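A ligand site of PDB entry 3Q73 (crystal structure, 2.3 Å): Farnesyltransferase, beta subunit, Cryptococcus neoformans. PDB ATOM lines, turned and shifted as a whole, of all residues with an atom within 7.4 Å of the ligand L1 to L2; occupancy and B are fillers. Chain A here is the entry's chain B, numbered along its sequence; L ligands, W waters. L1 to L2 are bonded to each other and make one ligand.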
ATOM      1  N   ALA A   2     -18.360 -16.048 -24.649  1.00  0.00           N
ATOM      2  CA  ALA A   2     -19.399 -15.956 -25.720  1.00  0.00           C
ATOM      3  C   ALA A   2     -20.695 -15.295 -25.238  1.00  0.00           C
ATOM      4  O   ALA A   2     -21.469 -14.756 -26.047  1.00  0.00           O
ATOM      5  CB  ALA A   2     -19.688 -17.327 -26.301  1.00  0.00           C
ATOM      6  N   THR A   3     -20.921 -15.327 -23.932  1.00  0.00           N
ATOM      7  CA  THR A   3     -22.116 -14.747 -23.311  1.00  0.00           C
ATOM      8  C   THR A   3     -21.826 -13.444 -22.558  1.00  0.00           C
ATOM      9  O   THR A   3     -22.677 -12.944 -21.797  1.00  0.00           O
ATOM     10  CB  THR A   3     -22.801 -15.746 -22.350  1.00  0.00           C
ATOM     11  OG1 THR A   3     -21.876 -16.154 -21.337  1.00  0.00           O
ATOM     12  CG2 THR A   3     -23.323 -16.978 -23.105  1.00  0.00           C
ATOM     13  N   THR A   6     -24.177 -10.843 -23.710  1.00  0.00           N
ATOM     14  CA  THR A   6     -25.552 -11.339 -23.738  1.00  0.00           C
ATOM     15  C   THR A   6     -25.972 -11.862 -22.367  1.00  0.00           C
ATOM     16  O   THR A   6     -26.074 -13.074 -22.166  1.00  0.00           O
ATOM     17  CB  THR A   6     -25.737 -12.468 -24.780  1.00  0.00           C
ATOM     18  OG1 THR A   6     -24.756 -13.487 -24.578  1.00  0.00           O
ATOM     19  CG2 THR A   6     -25.625 -11.925 -26.181  1.00  0.00           C
ATOM     20  N   ASP A  46     -34.248 -21.081 -13.661  1.00  0.00           N
ATOM     21  CA  ASP A  46     -33.265 -20.465 -14.546  1.00  0.00           C
ATOM     22  C   ASP A  46     -32.696 -21.556 -15.469  1.00  0.00           C
ATOM     23  O   ASP A  46     -32.151 -22.539 -14.984  1.00  0.00           O
ATOM     24  CB  ASP A  46     -32.175 -19.811 -13.685  1.00  0.00           C
ATOM     25  CG  ASP A  46     -31.059 -19.159 -14.492  1.00  0.00           C
ATOM     26  OD1 ASP A  46     -31.079 -19.145 -15.748  1.00  0.00           O
ATOM     27  OD2 ASP A  46     -30.133 -18.645 -13.846  1.00  0.00           O
ATOM     28  N   PRO A  47     -32.866 -21.391 -16.799  1.00  0.00           N
ATOM     29  CA  PRO A  47     -32.367 -22.405 -17.741  1.00  0.00           C
ATOM     30  C   PRO A  47     -30.855 -22.598 -17.670  1.00  0.00           C
ATOM     31  O   PRO A  47     -30.359 -23.684 -17.977  1.00  0.00           O
ATOM     32  CB  PRO A  47     -32.763 -21.837 -19.109  1.00  0.00           C
ATOM     33  CG  PRO A  47     -33.856 -20.877 -18.838  1.00  0.00           C
ATOM     34  CD  PRO A  47     -33.580 -20.308 -17.483  1.00  0.00           C
ATOM     35  N   ASN A  48     -30.121 -21.554 -17.268  1.00  0.00           N
ATOM     36  CA  ASN A  48     -28.659 -21.583 -17.221  1.00  0.00           C
ATOM     37  C   ASN A  48     -28.077 -22.332 -16.015  1.00  0.00           C
ATOM     38  O   ASN A  48     -26.878 -22.640 -15.997  1.00  0.00           O
ATOM     39  CB  ASN A  48     -28.093 -20.156 -17.260  1.00  0.00           C
ATOM     40  CG  ASN A  48     -28.566 -19.377 -18.475  1.00  0.00           C
ATOM     41  OD1 ASN A  48     -28.000 -19.492 -19.566  1.00  0.00           O
ATOM     42  ND2 ASN A  48     -29.587 -18.552 -18.292  1.00  0.00           N
ATOM     43  N   ALA A  49     -28.906 -22.620 -15.022  1.00  0.00           N
ATOM     44  CA  ALA A  49     -28.449 -23.221 -13.762  1.00  0.00           C
ATOM     45  C   ALA A  49     -28.067 -24.688 -13.876  1.00  0.00           C
ATOM     46  O   ALA A  49     -28.642 -25.434 -14.675  1.00  0.00           O
ATOM     47  CB  ALA A  49     -29.509 -23.030 -12.676  1.00  0.00           C
ATOM     48  N   LEU A  50     -27.068 -25.085 -13.091  1.00  0.00           N
ATOM     49  CA  LEU A  50     -26.722 -26.499 -12.903  1.00  0.00           C
ATOM     50  C   LEU A  50     -27.662 -27.105 -11.872  1.00  0.00           C
ATOM     51  O   LEU A  50     -28.271 -28.148 -12.124  1.00  0.00           O
ATOM     52  CB  LEU A  50     -25.269 -26.650 -12.428  1.00  0.00           C
ATOM     53  CG  LEU A  50     -24.110 -26.528 -13.416  1.00  0.00           C
ATOM     54  CD1 LEU A  50     -22.782 -26.478 -12.659  1.00  0.00           C
ATOM     55  CD2 LEU A  50     -24.111 -27.660 -14.456  1.00  0.00           C
ATOM     56  N   VAL A 378     -29.135 -14.584 -25.658  1.00  0.00           N
ATOM     57  CA  VAL A 378     -29.488 -15.413 -24.505  1.00  0.00           C
ATOM     58  C   VAL A 378     -30.894 -15.092 -23.986  1.00  0.00           C
ATOM     59  O   VAL A 378     -31.715 -16.005 -23.821  1.00  0.00           O
ATOM     60  CB  VAL A 378     -28.406 -15.319 -23.376  1.00  0.00           C
ATOM     61  CG1 VAL A 378     -28.910 -15.922 -22.068  1.00  0.00           C
ATOM     62  CG2 VAL A 378     -27.116 -15.990 -23.810  1.00  0.00           C
ATOM     63  N   GLN A 381     -33.802 -16.418 -26.138  1.00  0.00           N
ATOM     64  CA  GLN A 381     -34.039 -17.855 -25.930  1.00  0.00           C
ATOM     65  C   GLN A 381     -34.782 -18.069 -24.619  1.00  0.00           C
ATOM     66  O   GLN A 381     -35.683 -18.900 -24.548  1.00  0.00           O
ATOM     67  CB  GLN A 381     -32.732 -18.633 -25.926  1.00  0.00           C
ATOM     68  CG  GLN A 381     -31.959 -18.517 -27.227  1.00  0.00           C
ATOM     69  CD  GLN A 381     -30.738 -19.397 -27.249  1.00  0.00           C
ATOM     70  OE1 GLN A 381     -29.673 -18.966 -27.670  1.00  0.00           O
ATOM     71  NE2 GLN A 381     -30.884 -20.634 -26.794  1.00  0.00           N
ATOM     72  N   GLU A 382     -34.420 -17.295 -23.607  1.00  0.00           N
ATOM     73  CA  GLU A 382     -35.096 -17.331 -22.324  1.00  0.00           C
ATOM     74  C   GLU A 382     -36.573 -16.945 -22.438  1.00  0.00           C
ATOM     75  O   GLU A 382     -37.421 -17.578 -21.807  1.00  0.00           O
ATOM     76  CB  GLU A 382     -34.367 -16.459 -21.307  1.00  0.00           C
ATOM     77  CG  GLU A 382     -33.066 -17.081 -20.863  1.00  0.00           C
ATOM     78  CD  GLU A 382     -32.262 -16.200 -19.951  1.00  0.00           C
ATOM     79  OE1 GLU A 382     -32.350 -14.959 -20.066  1.00  0.00           O
ATOM     80  OE2 GLU A 382     -31.520 -16.768 -19.118  1.00  0.00           O
ATOM     81  N   GLN A 422     -30.223 -18.952 -31.418  1.00  0.00           N
ATOM     82  CA  GLN A 422     -29.369 -20.101 -31.107  1.00  0.00           C
ATOM     83  C   GLN A 422     -28.106 -20.173 -31.956  1.00  0.00           C
ATOM     84  O   GLN A 422     -27.045 -20.585 -31.463  1.00  0.00           O
ATOM     85  CB  GLN A 422     -30.131 -21.410 -31.249  1.00  0.00           C
ATOM     86  CG  GLN A 422     -31.040 -21.728 -30.075  1.00  0.00           C
ATOM     87  CD  GLN A 422     -31.628 -23.111 -30.148  1.00  0.00           C
ATOM     88  OE1 GLN A 422     -31.475 -23.834 -31.144  1.00  0.00           O
ATOM     89  NE2 GLN A 422     -32.316 -23.510 -29.087  1.00  0.00           N
ATOM     90  N   GLY A 482     -18.244 -21.977 -33.907  1.00  0.00           N
ATOM     91  CA  GLY A 482     -18.135 -21.504 -32.529  1.00  0.00           C
ATOM     92  C   GLY A 482     -19.147 -20.433 -32.129  1.00  0.00           C
ATOM     93  O   GLY A 482     -19.101 -19.918 -31.019  1.00  0.00           O
ATOM     94  N   GLY A 483     -20.054 -20.100 -33.049  1.00  0.00           N
ATOM     95  CA  GLY A 483     -21.049 -19.064 -32.810  1.00  0.00           C
ATOM     96  C   GLY A 483     -22.320 -19.552 -32.133  1.00  0.00           C
ATOM     97  O   GLY A 483     -23.211 -18.764 -31.810  1.00  0.00           O
ATOM     98  N   GLU A 484     -22.394 -20.867 -31.897  1.00  0.00           N
ATOM     99  CA  GLU A 484     -23.580 -21.490 -31.324  1.00  0.00           C
ATOM    100  C   GLU A 484     -23.722 -21.238 -29.814  1.00  0.00           C
ATOM    101  O   GLU A 484     -22.784 -21.440 -29.049  1.00  0.00           O
ATOM    102  CB  GLU A 484     -23.572 -22.989 -31.608  1.00  0.00           C
ATOM    103  CG  GLU A 484     -24.945 -23.619 -31.532  1.00  0.00           C
ATOM    104  CD  GLU A 484     -24.913 -25.139 -31.571  1.00  0.00           C
ATOM    105  OE1 GLU A 484     -25.601 -25.729 -32.437  1.00  0.00           O
ATOM    106  OE2 GLU A 484     -24.210 -25.744 -30.733  1.00  0.00           O
ATOM    107  N   ILE A 485     -24.904 -20.782 -29.412  1.00  0.00           N
ATOM    108  CA  ILE A 485     -25.247 -20.672 -28.005  1.00  0.00           C
ATOM    109  C   ILE A 485     -26.616 -21.310 -27.792  1.00  0.00           C
ATOM    110  O   ILE A 485     -27.623 -20.794 -28.275  1.00  0.00           O
ATOM    111  CB  ILE A 485     -25.297 -19.197 -27.504  1.00  0.00           C
ATOM    112  CG1 ILE A 485     -23.955 -18.479 -27.751  1.00  0.00           C
ATOM    113  CG2 ILE A 485     -25.647 -19.145 -26.026  1.00  0.00           C
ATOM    114  CD1 ILE A 485     -24.053 -16.965 -27.718  1.00  0.00           C
ATOM    115  N   ILE A 486     -26.637 -22.435 -27.091  1.00  0.00           N
ATOM    116  CA  ILE A 486     -27.893 -23.124 -26.794  1.00  0.00           C
ATOM    117  C   ILE A 486     -28.215 -23.021 -25.302  1.00  0.00           C
ATOM    118  O   ILE A 486     -27.738 -23.818 -24.484  1.00  0.00           O
ATOM    119  CB  ILE A 486     -27.886 -24.613 -27.253  1.00  0.00           C
ATOM    120  CG1 ILE A 486     -27.240 -24.771 -28.635  1.00  0.00           C
ATOM    121  CG2 ILE A 486     -29.308 -25.183 -27.205  1.00  0.00           C
ATOM    122  CD1 ILE A 486     -28.016 -24.155 -29.790  1.00  0.00           C
ATOM    123  N   VAL A 487     -29.038 -22.028 -24.966  1.00  0.00           N
ATOM    124  CA  VAL A 487     -29.435 -21.768 -23.586  1.00  0.00           C
ATOM    125  C   VAL A 487     -30.188 -22.978 -23.039  1.00  0.00           C
ATOM    126  O   VAL A 487     -31.118 -23.479 -23.675  1.00  0.00           O
ATOM    127  CB  VAL A 487     -30.284 -20.480 -23.489  1.00  0.00           C
ATOM    128  CG1 VAL A 487     -30.897 -20.303 -22.091  1.00  0.00           C
ATOM    129  CG2 VAL A 487     -29.453 -19.262 -23.875  1.00  0.00           C
ATOM    130  N   GLY A 488     -29.750 -23.464 -21.884  1.00  0.00           N
ATOM    131  CA  GLY A 488     -30.399 -24.586 -21.202  1.00  0.00           C
ATOM    132  C   GLY A 488     -29.885 -25.962 -21.584  1.00  0.00           C
ATOM    133  O   GLY A 488     -30.393 -26.976 -21.093  1.00  0.00           O
ATOM    134  N   GLY A 489     -28.893 -26.009 -22.458  1.00  0.00           N
ATOM    135  CA  GLY A 489     -28.290 -27.283 -22.851  1.00  0.00           C
ATOM    136  C   GLY A 489     -28.677 -27.730 -24.247  1.00  0.00           C
ATOM    137  O   GLY A 489     -29.617 -27.188 -24.841  1.00  0.00           O
ATOM    138  N   LYS A 490     -27.969 -28.737 -24.751  1.00  0.00           N
ATOM    139  CA  LYS A 490     -28.089 -29.111 -26.162  1.00  0.00           C
ATOM    140  C   LYS A 490     -29.400 -29.788 -26.540  1.00  0.00           C
ATOM    141  O   LYS A 490     -29.747 -29.849 -27.714  1.00  0.00           O
ATOM    142  CB  LYS A 490     -26.885 -29.955 -26.598  1.00  0.00           C
ATOM    143  CG  LYS A 490     -25.582 -29.162 -26.609  1.00  0.00           C
ATOM    144  CD  LYS A 490     -24.408 -30.007 -27.045  1.00  0.00           C
ATOM    145  CE  LYS A 490     -23.193 -29.142 -27.304  1.00  0.00           C
ATOM    146  NZ  LYS A 490     -22.015 -29.933 -27.788  1.00  0.00           N
ATOM    147  N   ASP A 491     -30.154 -30.274 -25.555  1.00  0.00           N
ATOM    148  CA  ASP A 491     -31.490 -30.813 -25.830  1.00  0.00           C
ATOM    149  C   ASP A 491     -32.486 -29.731 -26.269  1.00  0.00           C
ATOM    150  O   ASP A 491     -33.525 -30.062 -26.835  1.00  0.00           O
ATOM    151  CB  ASP A 491     -32.032 -31.591 -24.628  1.00  0.00           C
ATOM    152  CG  ASP A 491     -31.352 -32.926 -24.449  1.00  0.00           C
ATOM    153  OD1 ASP A 491     -31.033 -33.606 -25.458  1.00  0.00           O
ATOM    154  OD2 ASP A 491     -31.135 -33.308 -23.285  1.00  0.00           O
ATOM    155  N   ASN A 492     -32.172 -28.467 -26.002  1.00  0.00           N
ATOM    156  CA  ASN A 492     -32.989 -27.347 -26.482  1.00  0.00           C
ATOM    157  C   ASN A 492     -32.705 -26.954 -27.937  1.00  0.00           C
ATOM    158  O   ASN A 492     -33.469 -26.195 -28.544  1.00  0.00           O
ATOM    159  CB  ASN A 492     -32.845 -26.130 -25.567  1.00  0.00           C
ATOM    160  CG  ASN A 492     -33.494 -26.335 -24.213  1.00  0.00           C
ATOM    161  OD1 ASN A 492     -34.368 -27.188 -24.038  1.00  0.00           O
ATOM    162  ND2 ASN A 492     -33.070 -25.537 -23.239  1.00  0.00           N
ATOM    163  N   ARG A 493     -31.615 -27.476 -28.489  1.00  0.00           N
ATOM    164  CA  ARG A 493     -31.192 -27.118 -29.850  1.00  0.00           C
ATOM    165  C   ARG A 493     -32.253 -27.422 -30.887  1.00  0.00           C
ATOM    166  O   ARG A 493     -32.815 -28.517 -30.913  1.00  0.00           O
ATOM    167  CB  ARG A 493     -29.881 -27.810 -30.239  1.00  0.00           C
ATOM    168  CG  ARG A 493     -29.393 -27.414 -31.635  1.00  0.00           C
ATOM    169  CD  ARG A 493     -28.285 -28.334 -32.144  1.00  0.00           C
ATOM    170  NE  ARG A 493     -27.763 -27.851 -33.427  1.00  0.00           N
ATOM    171  CZ  ARG A 493     -28.298 -28.121 -34.614  1.00  0.00           C
ATOM    172  NH1 ARG A 493     -29.394 -28.875 -34.712  1.00  0.00           N
ATOM    173  NH2 ARG A 493     -27.752 -27.625 -35.715  1.00  0.00           N
HETATM  174  C1  LIG L   1     -24.085 -24.031 -21.556  1.00  0.00           C
HETATM  175  C2  LIG L   1     -24.981 -24.433 -20.413  1.00  0.00           C
HETATM  176  C3  LIG L   1     -25.926 -23.436 -19.810  1.00  0.00           C
HETATM  177  C4  LIG L   1     -26.223 -22.189 -20.561  1.00  0.00           C
HETATM  178  C5  LIG L   1     -25.482 -22.195 -21.882  1.00  0.00           C
HETATM  179  C6  LIG L   1     -25.426 -20.810 -22.424  1.00  0.00           C
HETATM  180  O1  LIG L   1     -24.879 -25.705 -19.901  1.00  0.00           O
HETATM  181  O2  LIG L   1     -26.598 -23.759 -18.641  1.00  0.00           O
HETATM  182  O3  LIG L   1     -27.591 -22.040 -20.774  1.00  0.00           O
HETATM  183  O4  LIG L   1     -24.147 -22.645 -21.815  1.00  0.00           O
HETATM  184  O5  LIG L   1     -24.573 -20.012 -21.686  1.00  0.00           O
HETATM  185  C1  LG2 L   2     -23.122 -26.642 -23.038  1.00  0.00           C
HETATM  186  C2  LG2 L   2     -23.574 -25.302 -23.523  1.00  0.00           C
HETATM  187  C3  LG2 L   2     -24.316 -25.365 -24.817  1.00  0.00           C
HETATM  188  C4  LG2 L   2     -23.785 -24.324 -25.726  1.00  0.00           C
HETATM  189  C5  LG2 L   2     -22.723 -23.675 -24.916  1.00  0.00           C
HETATM  190  C6  LG2 L   2     -21.860 -22.523 -25.369  1.00  0.00           C
HETATM  191  O1  LG2 L   2     -22.253 -27.216 -23.946  1.00  0.00           O
HETATM  192  O2  LG2 L   2     -24.541 -24.794 -22.623  1.00  0.00           O
HETATM  193  O3  LG2 L   2     -25.473 -26.107 -25.075  1.00  0.00           O
HETATM  194  O4  LG2 L   2     -24.403 -24.028 -26.953  1.00  0.00           O
HETATM  195  O5  LG2 L   2     -22.479 -24.423 -23.727  1.00  0.00           O
HETATM  196  O6  LG2 L   2     -21.929 -21.560 -24.370  1.00  0.00           O
HETATM  197  O1  LG3 L   3     -24.160 -30.970 -22.090  1.00  0.00           O
HETATM  198  O2  LG3 L   3     -25.625 -31.646 -23.869  1.00  0.00           O
HETATM  199  O3  LG3 L   3     -28.453 -31.755 -22.990  1.00  0.00           O
HETATM  200  O4  LG3 L   3     -25.897 -29.500 -22.847  1.00  0.00           O
HETATM  201  C1  LG3 L   3     -33.462 -34.221 -19.022  1.00  0.00           C
HETATM  202  C2  LG3 L   3     -32.041 -34.618 -18.771  1.00  0.00           C
HETATM  203  C3  LG3 L   3     -33.614 -32.749 -19.251  1.00  0.00           C
HETATM  204  C4  LG3 L   3     -31.102 -34.067 -19.792  1.00  0.00           C
HETATM  205  C5  LG3 L   3     -32.690 -32.247 -20.300  1.00  0.00           C
HETATM  206  C6  LG3 L   3     -29.107 -31.837 -20.716  1.00  0.00           C
HETATM  207  C7  LG3 L   3     -26.663 -31.590 -21.449  1.00  0.00           C
HETATM  208  N1  LG3 L   3     -30.464 -32.094 -21.107  1.00  0.00           N
HETATM  209  C8  LG3 L   3     -28.104 -31.681 -21.814  1.00  0.00           C
HETATM  210  C9  LG3 L   3     -31.277 -32.587 -20.001  1.00  0.00           C
HETATM  211  S1  LG3 L   3     -25.528 -30.901 -22.611  1.00  0.00           S
HETATM  212  O   HOH W   1     -21.421 -25.823 -19.807  1.00  0.00           O
HETATM  213  O   HOH W   2     -27.805 -26.168 -18.801  1.00  0.00           O
HETATM  214  O   HOH W   3     -23.131 -25.907 -28.364  1.00  0.00           O
HETATM  215  O   HOH W   4     -26.149 -28.098 -20.476  1.00  0.00           O
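An oxygen (O4) of LG2 L2 lies within hydrogen-bond range of the backbone NH (N) of Ile 486 (2.7 Å). O of Ile 486 sits at hydrogen-bond distance from O3 of LG2 L2, at 3.3 Å. The backbone NH (N) of Gly 488 is in hydrogen-bond range of an oxygen (O3) of LIG L1 (2.8 Å). An oxygen (O2) of LIG L1 lies within hydrogen-bond range of the backbone carbonyl oxygen (O) of Asn 48 (2.9 Å). OD1 of Asn 48 is in hydrogen-bond range of O3 of LIG L1, at 2.8 Å. The backbone NH (N) of Lys 490 is in hydrogen-bond range of an oxygen (O4) of LG3 L3 (2.9 Å). An oxygen (O3) of LG3 L3 sits at hydrogen-bond distance from the backbone NH (N) of Asp 491. The side-chain carboxylate (OD2) of Asp 491 lies within salt-bridge range of a nitrogen (N1) of LG3 L3 (2.6 Å).
The backbone NH (N) of Asn 48 sits at hydrogen-bond distance from the side-chain carboxylate (OD1) of Asp 46. The side-chain carboxylate (OE2) of Glu 382 is in hydrogen-bond range of the side-chain amide nitrogen (ND2) of Asn 48, 2.8 Å away. The backbone carbonyl oxygen (O) of Val 487 lies within hydrogen-bond range of the side-chain amide nitrogen (ND2) of Asn 492 (2.9 Å). The side-chain amide nitrogen (NE2) of Gln 381 lies close to the backbone NH (N) of Val 487 (2.9 Å). N of Ile 485 is in hydrogen-bond range of O of Gln 422 (3.0 Å). OE1 of Gln 381 sits close to O of Ile 485, 2.8 Å away. NE of Arg 493 lies within salt-bridge range of OE1 of Glu 484 (3.2 Å).
Thr 3 touches the ligand L1 to L2. Pro 47 touches the ligand L1 to L2. Glu 484 touches the ligand L1 to L2. C of Ile 485 touches O4 of LG2 L2, 3.6 Å away. CA of Val 487 touches O3 of LIG L1, at 3.4 Å. C of Gly 489 touches O3 of LG2 L2, at 3.7 Å. CG of Lys 490 touches O3 of LG2 L2, 3.4 Å away. Hydrophobic or aromatic side chains that line the ligand L1 to L2: Ile 485, Ile 486 and Val 487. Of the 24 residues printed, 10 come within 4 Å of the ligand L1 to L2.
Water W3 bridges OE2 of Glu 484 (2.6 Å) and O4 of LG2 L2 (2.7 Å). Water W4 lies within hydrogen-bond range of O4 of LG3 L3 and O1 of LIG L1.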
